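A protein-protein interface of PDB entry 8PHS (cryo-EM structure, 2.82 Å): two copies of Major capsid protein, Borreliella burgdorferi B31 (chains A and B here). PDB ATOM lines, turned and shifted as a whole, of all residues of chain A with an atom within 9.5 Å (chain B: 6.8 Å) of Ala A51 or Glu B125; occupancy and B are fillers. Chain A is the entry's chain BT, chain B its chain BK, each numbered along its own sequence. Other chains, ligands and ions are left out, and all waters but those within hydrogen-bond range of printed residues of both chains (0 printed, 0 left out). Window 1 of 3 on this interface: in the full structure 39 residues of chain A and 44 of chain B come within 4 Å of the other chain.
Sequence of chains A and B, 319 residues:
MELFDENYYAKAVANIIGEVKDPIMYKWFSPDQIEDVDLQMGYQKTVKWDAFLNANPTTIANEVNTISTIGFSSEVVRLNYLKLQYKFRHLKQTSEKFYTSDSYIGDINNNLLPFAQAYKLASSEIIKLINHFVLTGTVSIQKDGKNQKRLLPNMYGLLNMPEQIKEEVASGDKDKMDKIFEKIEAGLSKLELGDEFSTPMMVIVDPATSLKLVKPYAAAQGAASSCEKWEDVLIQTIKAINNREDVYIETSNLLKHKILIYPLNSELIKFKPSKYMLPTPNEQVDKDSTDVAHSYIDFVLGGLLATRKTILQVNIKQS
Ala A51 touches just these residues of chain B: Leu B121 (3.6 Å) and Glu B125 (3.2 Å).
No residue of chain A comes within 4 Å of Lys B128.
Printed residues of chain B within 4 Å of Trp A49: Leu B121 (3.9 Å).
Of the printed residues of chain A, Leu B121 touches Trp A49 (3.9 Å), Ala A51 (3.6 Å) and Phe A72 (3.9 Å).
Of the printed residues of chain B, Ile A70 touches Ala B122.
Of the printed residues of chain B, Phe A72 touches Ala B118 and Leu B121.
Of the printed residues of chain A, Ala B122 touches Ile A70 (3.8 Å).
Lys B120 touches none of the printed residues of chain A.
Leu A53 touches none of the printed residues of chain B.
The nearest residue of chain B that does not touch Ala A51 is Ala B122 (4.3 Å).
The nearest residue of chain A that does not touch Glu B125 is Leu A53 (4.05 Å).
No position is printed for both chains.
Of the 6 pairs that touch across the chains among the printed residues, none has its exchanged pair printed and touching as well.
The backbone carbonyl oxygen (O) of Ala A51 lies close to the side-chain carboxylate (OE1) of Glu B125 (3.4 Å).
The side-chain amino group of Lys B128 is in salt-bridge range of the side-chain carboxylate of Glu B125, at 3.5 Å.
Of the 16 printed residues of chain A, 4 touch a printed residue of chain B.
Hydrophobic or aromatic side chains of chain A that line the printed part of chain B: Trp A49, Ala A51, Ile A70 and Phe A72.
Of the 13 printed residues of chain B, 4 touch a printed residue of chain A.
Among the printed residues, 6 pairs touch across the chains.
Among the printed residues, no Asp or Glu carboxylate lies within 4 Å of a Lys or Arg side-chain nitrogen of the other chain.
Among the printed residues, pairs that only touch across the chains: Phe A72 with Ala B118, Ala A51 with Leu B121, Ile A70 with Ala B122, Phe A72 with Leu B121 and Trp A49 with Leu B121.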
ATOM      1  N   LYS A  48      -7.328   9.037 -17.433  1.00  0.00           N
ATOM      2  CA  LYS A  48      -6.455   9.405 -18.537  1.00  0.00           C
ATOM      3  C   LYS A  48      -6.514  10.911 -18.739  1.00  0.00           C
ATOM      4  O   LYS A  48      -7.600  11.481 -18.890  1.00  0.00           O
ATOM      5  CB  LYS A  48      -6.854   8.680 -19.822  1.00  0.00           C
ATOM      6  CG  LYS A  48      -5.893   8.912 -20.974  1.00  0.00           C
ATOM      7  CD  LYS A  48      -6.416   8.310 -22.263  1.00  0.00           C
ATOM      8  CE  LYS A  48      -5.373   8.390 -23.363  1.00  0.00           C
ATOM      9  NZ  LYS A  48      -5.859   7.785 -24.634  1.00  0.00           N
ATOM     10  N   TRP A  49      -5.350  11.549 -18.744  1.00  0.00           N
ATOM     11  CA  TRP A  49      -5.247  12.992 -18.895  1.00  0.00           C
ATOM     12  C   TRP A  49      -4.805  13.336 -20.310  1.00  0.00           C
ATOM     13  O   TRP A  49      -3.943  12.662 -20.883  1.00  0.00           O
ATOM     14  CB  TRP A  49      -4.260  13.570 -17.880  1.00  0.00           C
ATOM     15  CG  TRP A  49      -4.752  13.520 -16.468  1.00  0.00           C
ATOM     16  CD1 TRP A  49      -4.456  12.574 -15.532  1.00  0.00           C
ATOM     17  CD2 TRP A  49      -5.620  14.461 -15.827  1.00  0.00           C
ATOM     18  NE1 TRP A  49      -5.087  12.864 -14.349  1.00  0.00           N
ATOM     19  CE2 TRP A  49      -5.808  14.019 -14.502  1.00  0.00           C
ATOM     20  CE3 TRP A  49      -6.258  15.632 -16.242  1.00  0.00           C
ATOM     21  CZ2 TRP A  49      -6.606  14.707 -13.593  1.00  0.00           C
ATOM     22  CZ3 TRP A  49      -7.049  16.314 -15.338  1.00  0.00           C
ATOM     23  CH2 TRP A  49      -7.216  15.849 -14.029  1.00  0.00           C
ATOM     24  N   ASP A  50      -5.400  14.384 -20.871  1.00  0.00           N
ATOM     25  CA  ASP A  50      -5.097  14.810 -22.229  1.00  0.00           C
ATOM     26  C   ASP A  50      -4.956  16.323 -22.270  1.00  0.00           C
ATOM     27  O   ASP A  50      -5.462  17.041 -21.404  1.00  0.00           O
ATOM     28  CB  ASP A  50      -6.176  14.358 -23.222  1.00  0.00           C
ATOM     29  CG  ASP A  50      -6.338  12.852 -23.264  1.00  0.00           C
ATOM     30  OD1 ASP A  50      -5.380  12.162 -23.673  1.00  0.00           O
ATOM     31  OD2 ASP A  50      -7.423  12.360 -22.892  1.00  0.00           O
ATOM     32  N   ALA A  51      -4.256  16.799 -23.296  1.00  0.00           N
ATOM     33  CA  ALA A  51      -4.084  18.220 -23.547  1.00  0.00           C
ATOM     34  C   ALA A  51      -4.481  18.526 -24.981  1.00  0.00           C
ATOM     35  O   ALA A  51      -4.363  17.678 -25.868  1.00  0.00           O
ATOM     36  CB  ALA A  51      -2.641  18.669 -23.298  1.00  0.00           C
ATOM     37  N   PHE A  52      -4.960  19.747 -25.202  1.00  0.00           N
ATOM     38  CA  PHE A  52      -5.394  20.178 -26.521  1.00  0.00           C
ATOM     39  C   PHE A  52      -5.001  21.632 -26.733  1.00  0.00           C
ATOM     40  O   PHE A  52      -4.781  22.383 -25.780  1.00  0.00           O
ATOM     41  CB  PHE A  52      -6.906  19.992 -26.707  1.00  0.00           C
ATOM     42  CG  PHE A  52      -7.737  20.617 -25.622  1.00  0.00           C
ATOM     43  CD1 PHE A  52      -8.158  21.932 -25.722  1.00  0.00           C
ATOM     44  CD2 PHE A  52      -8.097  19.888 -24.503  1.00  0.00           C
ATOM     45  CE1 PHE A  52      -8.924  22.506 -24.727  1.00  0.00           C
ATOM     46  CE2 PHE A  52      -8.860  20.457 -23.504  1.00  0.00           C
ATOM     47  CZ  PHE A  52      -9.275  21.767 -23.617  1.00  0.00           C
ATOM     48  N   LEU A  53      -4.911  22.018 -28.002  1.00  0.00           N
ATOM     49  CA  LEU A  53      -4.515  23.365 -28.391  1.00  0.00           C
ATOM     50  C   LEU A  53      -5.765  24.178 -28.703  1.00  0.00           C
ATOM     51  O   LEU A  53      -6.562  23.792 -29.564  1.00  0.00           O
ATOM     52  CB  LEU A  53      -3.582  23.324 -29.601  1.00  0.00           C
ATOM     53  CG  LEU A  53      -2.343  22.436 -29.472  1.00  0.00           C
ATOM     54  CD1 LEU A  53      -1.582  22.390 -30.784  1.00  0.00           C
ATOM     55  CD2 LEU A  53      -1.444  22.922 -28.349  1.00  0.00           C
ATOM     56  N   ASN A  54      -5.933  25.302 -28.002  1.00  0.00           N
ATOM     57  CA  ASN A  54      -7.118  26.127 -28.204  1.00  0.00           C
ATOM     58  C   ASN A  54      -7.057  26.906 -29.511  1.00  0.00           C
ATOM     59  O   ASN A  54      -8.086  27.075 -30.176  1.00  0.00           O
ATOM     60  CB  ASN A  54      -7.299  27.088 -27.031  1.00  0.00           C
ATOM     61  CG  ASN A  54      -7.559  26.369 -25.727  1.00  0.00           C
ATOM     62  OD1 ASN A  54      -6.750  26.421 -24.802  1.00  0.00           O
ATOM     63  ND2 ASN A  54      -8.697  25.695 -25.643  1.00  0.00           N
ATOM     64  N   PRO A  57      -0.465  29.124 -32.297  1.00  0.00           N
ATOM     65  CA  PRO A  57       0.508  29.719 -31.377  1.00  0.00           C
ATOM     66  C   PRO A  57       0.704  31.202 -31.654  1.00  0.00           C
ATOM     67  O   PRO A  57       0.457  31.701 -32.753  1.00  0.00           O
ATOM     68  CB  PRO A  57       1.791  28.927 -31.650  1.00  0.00           C
ATOM     69  CG  PRO A  57       1.614  28.386 -33.025  1.00  0.00           C
ATOM     70  CD  PRO A  57       0.151  28.107 -33.166  1.00  0.00           C
ATOM     71  N   THR A  69      -3.741  29.610 -25.471  1.00  0.00           N
ATOM     72  CA  THR A  69      -3.781  28.735 -24.313  1.00  0.00           C
ATOM     73  C   THR A  69      -3.795  27.270 -24.734  1.00  0.00           C
ATOM     74  O   THR A  69      -4.173  26.922 -25.855  1.00  0.00           O
ATOM     75  CB  THR A  69      -5.007  29.031 -23.442  1.00  0.00           C
ATOM     76  OG1 THR A  69      -6.184  29.037 -24.258  1.00  0.00           O
ATOM     77  CG2 THR A  69      -4.861  30.378 -22.760  1.00  0.00           C
ATOM     78  N   ILE A  70      -3.364  26.417 -23.809  1.00  0.00           N
ATOM     79  CA  ILE A  70      -3.406  24.967 -23.966  1.00  0.00           C
ATOM     80  C   ILE A  70      -4.325  24.416 -22.887  1.00  0.00           C
ATOM     81  O   ILE A  70      -4.080  24.624 -21.692  1.00  0.00           O
ATOM     82  CB  ILE A  70      -2.008  24.337 -23.869  1.00  0.00           C
ATOM     83  CG1 ILE A  70      -1.163  24.712 -25.085  1.00  0.00           C
ATOM     84  CG2 ILE A  70      -2.111  22.829 -23.731  1.00  0.00           C
ATOM     85  CD1 ILE A  70       0.243  24.166 -25.030  1.00  0.00           C
ATOM     86  N   GLY A  71      -5.382  23.719 -23.303  1.00  0.00           N
ATOM     87  CA  GLY A  71      -6.341  23.183 -22.362  1.00  0.00           C
ATOM     88  C   GLY A  71      -5.989  21.785 -21.886  1.00  0.00           C
ATOM     89  O   GLY A  71      -5.055  21.149 -22.368  1.00  0.00           O
ATOM     90  N   PHE A  72      -6.757  21.314 -20.908  1.00  0.00           N
ATOM     91  CA  PHE A  72      -6.579  19.985 -20.346  1.00  0.00           C
ATOM     92  C   PHE A  72      -7.938  19.339 -20.121  1.00  0.00           C
ATOM     93  O   PHE A  72      -8.945  20.024 -19.925  1.00  0.00           O
ATOM     94  CB  PHE A  72      -5.793  20.039 -19.033  1.00  0.00           C
ATOM     95  CG  PHE A  72      -4.369  20.480 -19.202  1.00  0.00           C
ATOM     96  CD1 PHE A  72      -3.415  19.610 -19.700  1.00  0.00           C
ATOM     97  CD2 PHE A  72      -3.987  21.769 -18.877  1.00  0.00           C
ATOM     98  CE1 PHE A  72      -2.105  20.016 -19.861  1.00  0.00           C
ATOM     99  CE2 PHE A  72      -2.680  22.180 -19.037  1.00  0.00           C
ATOM    100  CZ  PHE A  72      -1.739  21.303 -19.530  1.00  0.00           C
ATOM    101  N   SER A  73      -7.957  18.009 -20.149  1.00  0.00           N
ATOM    102  CA  SER A  73      -9.187  17.259 -19.944  1.00  0.00           C
ATOM    103  C   SER A  73      -8.846  15.903 -19.344  1.00  0.00           C
ATOM    104  O   SER A  73      -7.716  15.420 -19.453  1.00  0.00           O
ATOM    105  CB  SER A  73      -9.968  17.092 -21.252  1.00  0.00           C
ATOM    106  OG  SER A  73     -11.107  16.272 -21.061  1.00  0.00           O
ATOM    107  N   SER A  74      -9.841  15.293 -18.705  1.00  0.00           N
ATOM    108  CA  SER A  74      -9.665  14.000 -18.061  1.00  0.00           C
ATOM    109  C   SER A  74     -10.843  13.097 -18.390  1.00  0.00           C
ATOM    110  O   SER A  74     -11.968  13.561 -18.590  1.00  0.00           O
ATOM    111  CB  SER A  74      -9.526  14.138 -16.541  1.00  0.00           C
ATOM    112  OG  SER A  74     -10.654  14.788 -15.986  1.00  0.00           O
ATOM    113  N   GLU A  75     -10.567  11.797 -18.440  1.00  0.00           N
ATOM    114  CA  GLU A  75     -11.579  10.778 -18.671  1.00  0.00           C
ATOM    115  C   GLU A  75     -11.367   9.652 -17.670  1.00  0.00           C
ATOM    116  O   GLU A  75     -10.233   9.229 -17.435  1.00  0.00           O
ATOM    117  CB  GLU A  75     -11.514  10.243 -20.107  1.00  0.00           C
ATOM    118  CG  GLU A  75     -12.588   9.230 -20.446  1.00  0.00           C
ATOM    119  CD  GLU A  75     -12.237   8.400 -21.664  1.00  0.00           C
ATOM    120  OE1 GLU A  75     -11.201   8.683 -22.300  1.00  0.00           O
ATOM    121  OE2 GLU A  75     -12.996   7.463 -21.985  1.00  0.00           O
ATOM    122  N   ASP A 195      -3.143   8.425 -34.630  1.00  0.00           N
ATOM    123  CA  ASP A 195      -1.696   8.590 -34.650  1.00  0.00           C
ATOM    124  C   ASP A 195      -0.949   7.357 -34.163  1.00  0.00           C
ATOM    125  O   ASP A 195       0.273   7.286 -34.333  1.00  0.00           O
ATOM    126  CB  ASP A 195      -1.293   9.797 -33.800  1.00  0.00           C
ATOM    127  CG  ASP A 195      -1.710  11.115 -34.425  1.00  0.00           C
ATOM    128  OD1 ASP A 195      -2.244  11.095 -35.552  1.00  0.00           O
ATOM    129  OD2 ASP A 195      -1.506  12.169 -33.786  1.00  0.00           O
ATOM    130  N   ALA B 118       1.356  18.789 -16.486  1.00  0.00           N
ATOM    131  CA  ALA B 118       0.855  19.740 -17.472  1.00  0.00           C
ATOM    132  C   ALA B 118       1.911  20.046 -18.525  1.00  0.00           C
ATOM    133  O   ALA B 118       1.610  20.090 -19.726  1.00  0.00           O
ATOM    134  CB  ALA B 118       0.397  21.019 -16.774  1.00  0.00           C
ATOM    135  N   LYS B 120       4.426  18.122 -19.434  1.00  0.00           N
ATOM    136  CA  LYS B 120       4.640  16.955 -20.283  1.00  0.00           C
ATOM    137  C   LYS B 120       3.566  16.852 -21.363  1.00  0.00           C
ATOM    138  O   LYS B 120       3.872  16.644 -22.547  1.00  0.00           O
ATOM    139  CB  LYS B 120       4.682  15.692 -19.424  1.00  0.00           C
ATOM    140  CG  LYS B 120       5.040  14.433 -20.189  1.00  0.00           C
ATOM    141  CD  LYS B 120       4.386  13.210 -19.581  1.00  0.00           C
ATOM    142  CE  LYS B 120       4.869  12.988 -18.157  1.00  0.00           C
ATOM    143  NZ  LYS B 120       4.443  11.662 -17.631  1.00  0.00           N
ATOM    144  N   LEU B 121       2.298  17.016 -20.976  1.00  0.00           N
ATOM    145  CA  LEU B 121       1.218  16.936 -21.959  1.00  0.00           C
ATOM    146  C   LEU B 121       1.332  18.046 -23.003  1.00  0.00           C
ATOM    147  O   LEU B 121       1.186  17.800 -24.214  1.00  0.00           O
ATOM    148  CB  LEU B 121      -0.136  16.996 -21.252  1.00  0.00           C
ATOM    149  CG  LEU B 121      -0.413  15.905 -20.219  1.00  0.00           C
ATOM    150  CD1 LEU B 121      -1.819  16.034 -19.658  1.00  0.00           C
ATOM    151  CD2 LEU B 121      -0.209  14.533 -20.830  1.00  0.00           C
ATOM    152  N   ALA B 122       1.599  19.276 -22.555  1.00  0.00           N
ATOM    153  CA  ALA B 122       1.728  20.388 -23.487  1.00  0.00           C
ATOM    154  C   ALA B 122       2.905  20.182 -24.430  1.00  0.00           C
ATOM    155  O   ALA B 122       2.819  20.502 -25.622  1.00  0.00           O
ATOM    156  CB  ALA B 122       1.874  21.700 -22.718  1.00  0.00           C
ATOM    157  N   SER B 123       4.016  19.650 -23.914  1.00  0.00           N
ATOM    158  CA  SER B 123       5.172  19.378 -24.758  1.00  0.00           C
ATOM    159  C   SER B 123       4.840  18.349 -25.825  1.00  0.00           C
ATOM    160  O   SER B 123       5.252  18.493 -26.981  1.00  0.00           O
ATOM    161  CB  SER B 123       6.344  18.902 -23.901  1.00  0.00           C
ATOM    162  OG  SER B 123       6.701  19.876 -22.939  1.00  0.00           O
ATOM    163  N   SER B 124       4.096  17.302 -25.461  1.00  0.00           N
ATOM    164  CA  SER B 124       3.704  16.308 -26.458  1.00  0.00           C
ATOM    165  C   SER B 124       2.857  16.940 -27.559  1.00  0.00           C
ATOM    166  O   SER B 124       3.080  16.695 -28.755  1.00  0.00           O
ATOM    167  CB  SER B 124       2.953  15.159 -25.786  1.00  0.00           C
ATOM    168  OG  SER B 124       3.744  14.561 -24.774  1.00  0.00           O
ATOM    169  N   GLU B 125       1.886  17.773 -27.173  1.00  0.00           N
ATOM    170  CA  GLU B 125       1.044  18.422 -28.180  1.00  0.00           C
ATOM    171  C   GLU B 125       1.862  19.334 -29.093  1.00  0.00           C
ATOM    172  O   GLU B 125       1.676  19.340 -30.320  1.00  0.00           O
ATOM    173  CB  GLU B 125      -0.075  19.209 -27.500  1.00  0.00           C
ATOM    174  CG  GLU B 125      -1.063  18.342 -26.745  1.00  0.00           C
ATOM    175  CD  GLU B 125      -1.711  17.298 -27.633  1.00  0.00           C
ATOM    176  OE1 GLU B 125      -2.399  17.686 -28.600  1.00  0.00           O
ATOM    177  OE2 GLU B 125      -1.531  16.091 -27.365  1.00  0.00           O
ATOM    178  N   ILE B 126       2.783  20.106 -28.512  1.00  0.00           N
ATOM    179  CA  ILE B 126       3.587  21.024 -29.313  1.00  0.00           C
ATOM    180  C   ILE B 126       4.510  20.252 -30.247  1.00  0.00           C
ATOM    181  O   ILE B 126       4.754  20.673 -31.384  1.00  0.00           O
ATOM    182  CB  ILE B 126       4.364  21.988 -28.400  1.00  0.00           C
ATOM    183  CG1 ILE B 126       3.388  22.859 -27.608  1.00  0.00           C
ATOM    184  CG2 ILE B 126       5.288  22.872 -29.215  1.00  0.00           C
ATOM    185  CD1 ILE B 126       4.046  23.687 -26.532  1.00  0.00           C
ATOM    186  N   ILE B 127       5.033  19.111 -29.795  1.00  0.00           N
ATOM    187  CA  ILE B 127       5.881  18.292 -30.658  1.00  0.00           C
ATOM    188  C   ILE B 127       5.078  17.751 -31.833  1.00  0.00           C
ATOM    189  O   ILE B 127       5.573  17.689 -32.966  1.00  0.00           O
ATOM    190  CB  ILE B 127       6.545  17.164 -29.846  1.00  0.00           C
ATOM    191  CG1 ILE B 127       7.599  17.743 -28.902  1.00  0.00           C
ATOM    192  CG2 ILE B 127       7.172  16.135 -30.769  1.00  0.00           C
ATOM    193  CD1 ILE B 127       8.440  16.699 -28.207  1.00  0.00           C
ATOM    194  N   LYS B 128       3.827  17.352 -31.588  1.00  0.00           N
ATOM    195  CA  LYS B 128       2.977  16.931 -32.700  1.00  0.00           C
ATOM    196  C   LYS B 128       2.783  18.065 -33.702  1.00  0.00           C
ATOM    197  O   LYS B 128       2.853  17.852 -34.922  1.00  0.00           O
ATOM    198  CB  LYS B 128       1.627  16.439 -32.180  1.00  0.00           C
ATOM    199  CG  LYS B 128       1.705  15.183 -31.332  1.00  0.00           C
ATOM    200  CD  LYS B 128       0.334  14.791 -30.808  1.00  0.00           C
ATOM    201  CE  LYS B 128       0.423  13.606 -29.862  1.00  0.00           C
ATOM    202  NZ  LYS B 128      -0.910  13.246 -29.307  1.00  0.00           N
ATOM    203  N   LEU B 129       2.548  19.282 -33.203  1.00  0.00           N
ATOM    204  CA  LEU B 129       2.387  20.424 -34.103  1.00  0.00           C
ATOM    205  C   LEU B 129       3.659  20.682 -34.912  1.00  0.00           C
ATOM    206  O   LEU B 129       3.594  20.994 -36.109  1.00  0.00           O
ATOM    207  CB  LEU B 129       1.994  21.667 -33.308  1.00  0.00           C
ATOM    208  CG  LEU B 129       1.801  22.957 -34.107  1.00  0.00           C
ATOM    209  CD1 LEU B 129       0.633  22.823 -35.065  1.00  0.00           C
ATOM    210  CD2 LEU B 129       1.593  24.135 -33.172  1.00  0.00           C
ATOM    211  N   ILE B 130       4.822  20.564 -34.270  1.00  0.00           N
ATOM    212  CA  ILE B 130       6.091  20.776 -34.965  1.00  0.00           C
ATOM    213  C   ILE B 130       6.288  19.729 -36.054  1.00  0.00           C
ATOM    214  O   ILE B 130       6.758  20.038 -37.156  1.00  0.00           O
ATOM    215  CB  ILE B 130       7.260  20.777 -33.962  1.00  0.00           C
ATOM    216  CG1 ILE B 130       7.127  21.948 -32.989  1.00  0.00           C
ATOM    217  CG2 ILE B 130       8.590  20.847 -34.690  1.00  0.00           C
ATOM    218  CD1 ILE B 130       8.157  21.937 -31.886  1.00  0.00           C
ATOM    219  N   PRO B 279      10.121  22.084 -27.536  1.00  0.00           N
ATOM    220  CA  PRO B 279       9.534  22.934 -26.493  1.00  0.00           C
ATOM    221  C   PRO B 279      10.482  23.169 -25.325  1.00  0.00           C
ATOM    222  O   PRO B 279      11.196  22.267 -24.885  1.00  0.00           O
ATOM    223  CB  PRO B 279       8.297  22.145 -26.055  1.00  0.00           C
ATOM    224  CG  PRO B 279       7.911  21.383 -27.265  1.00  0.00           C
ATOM    225  CD  PRO B 279       9.196  21.013 -27.950  1.00  0.00           C
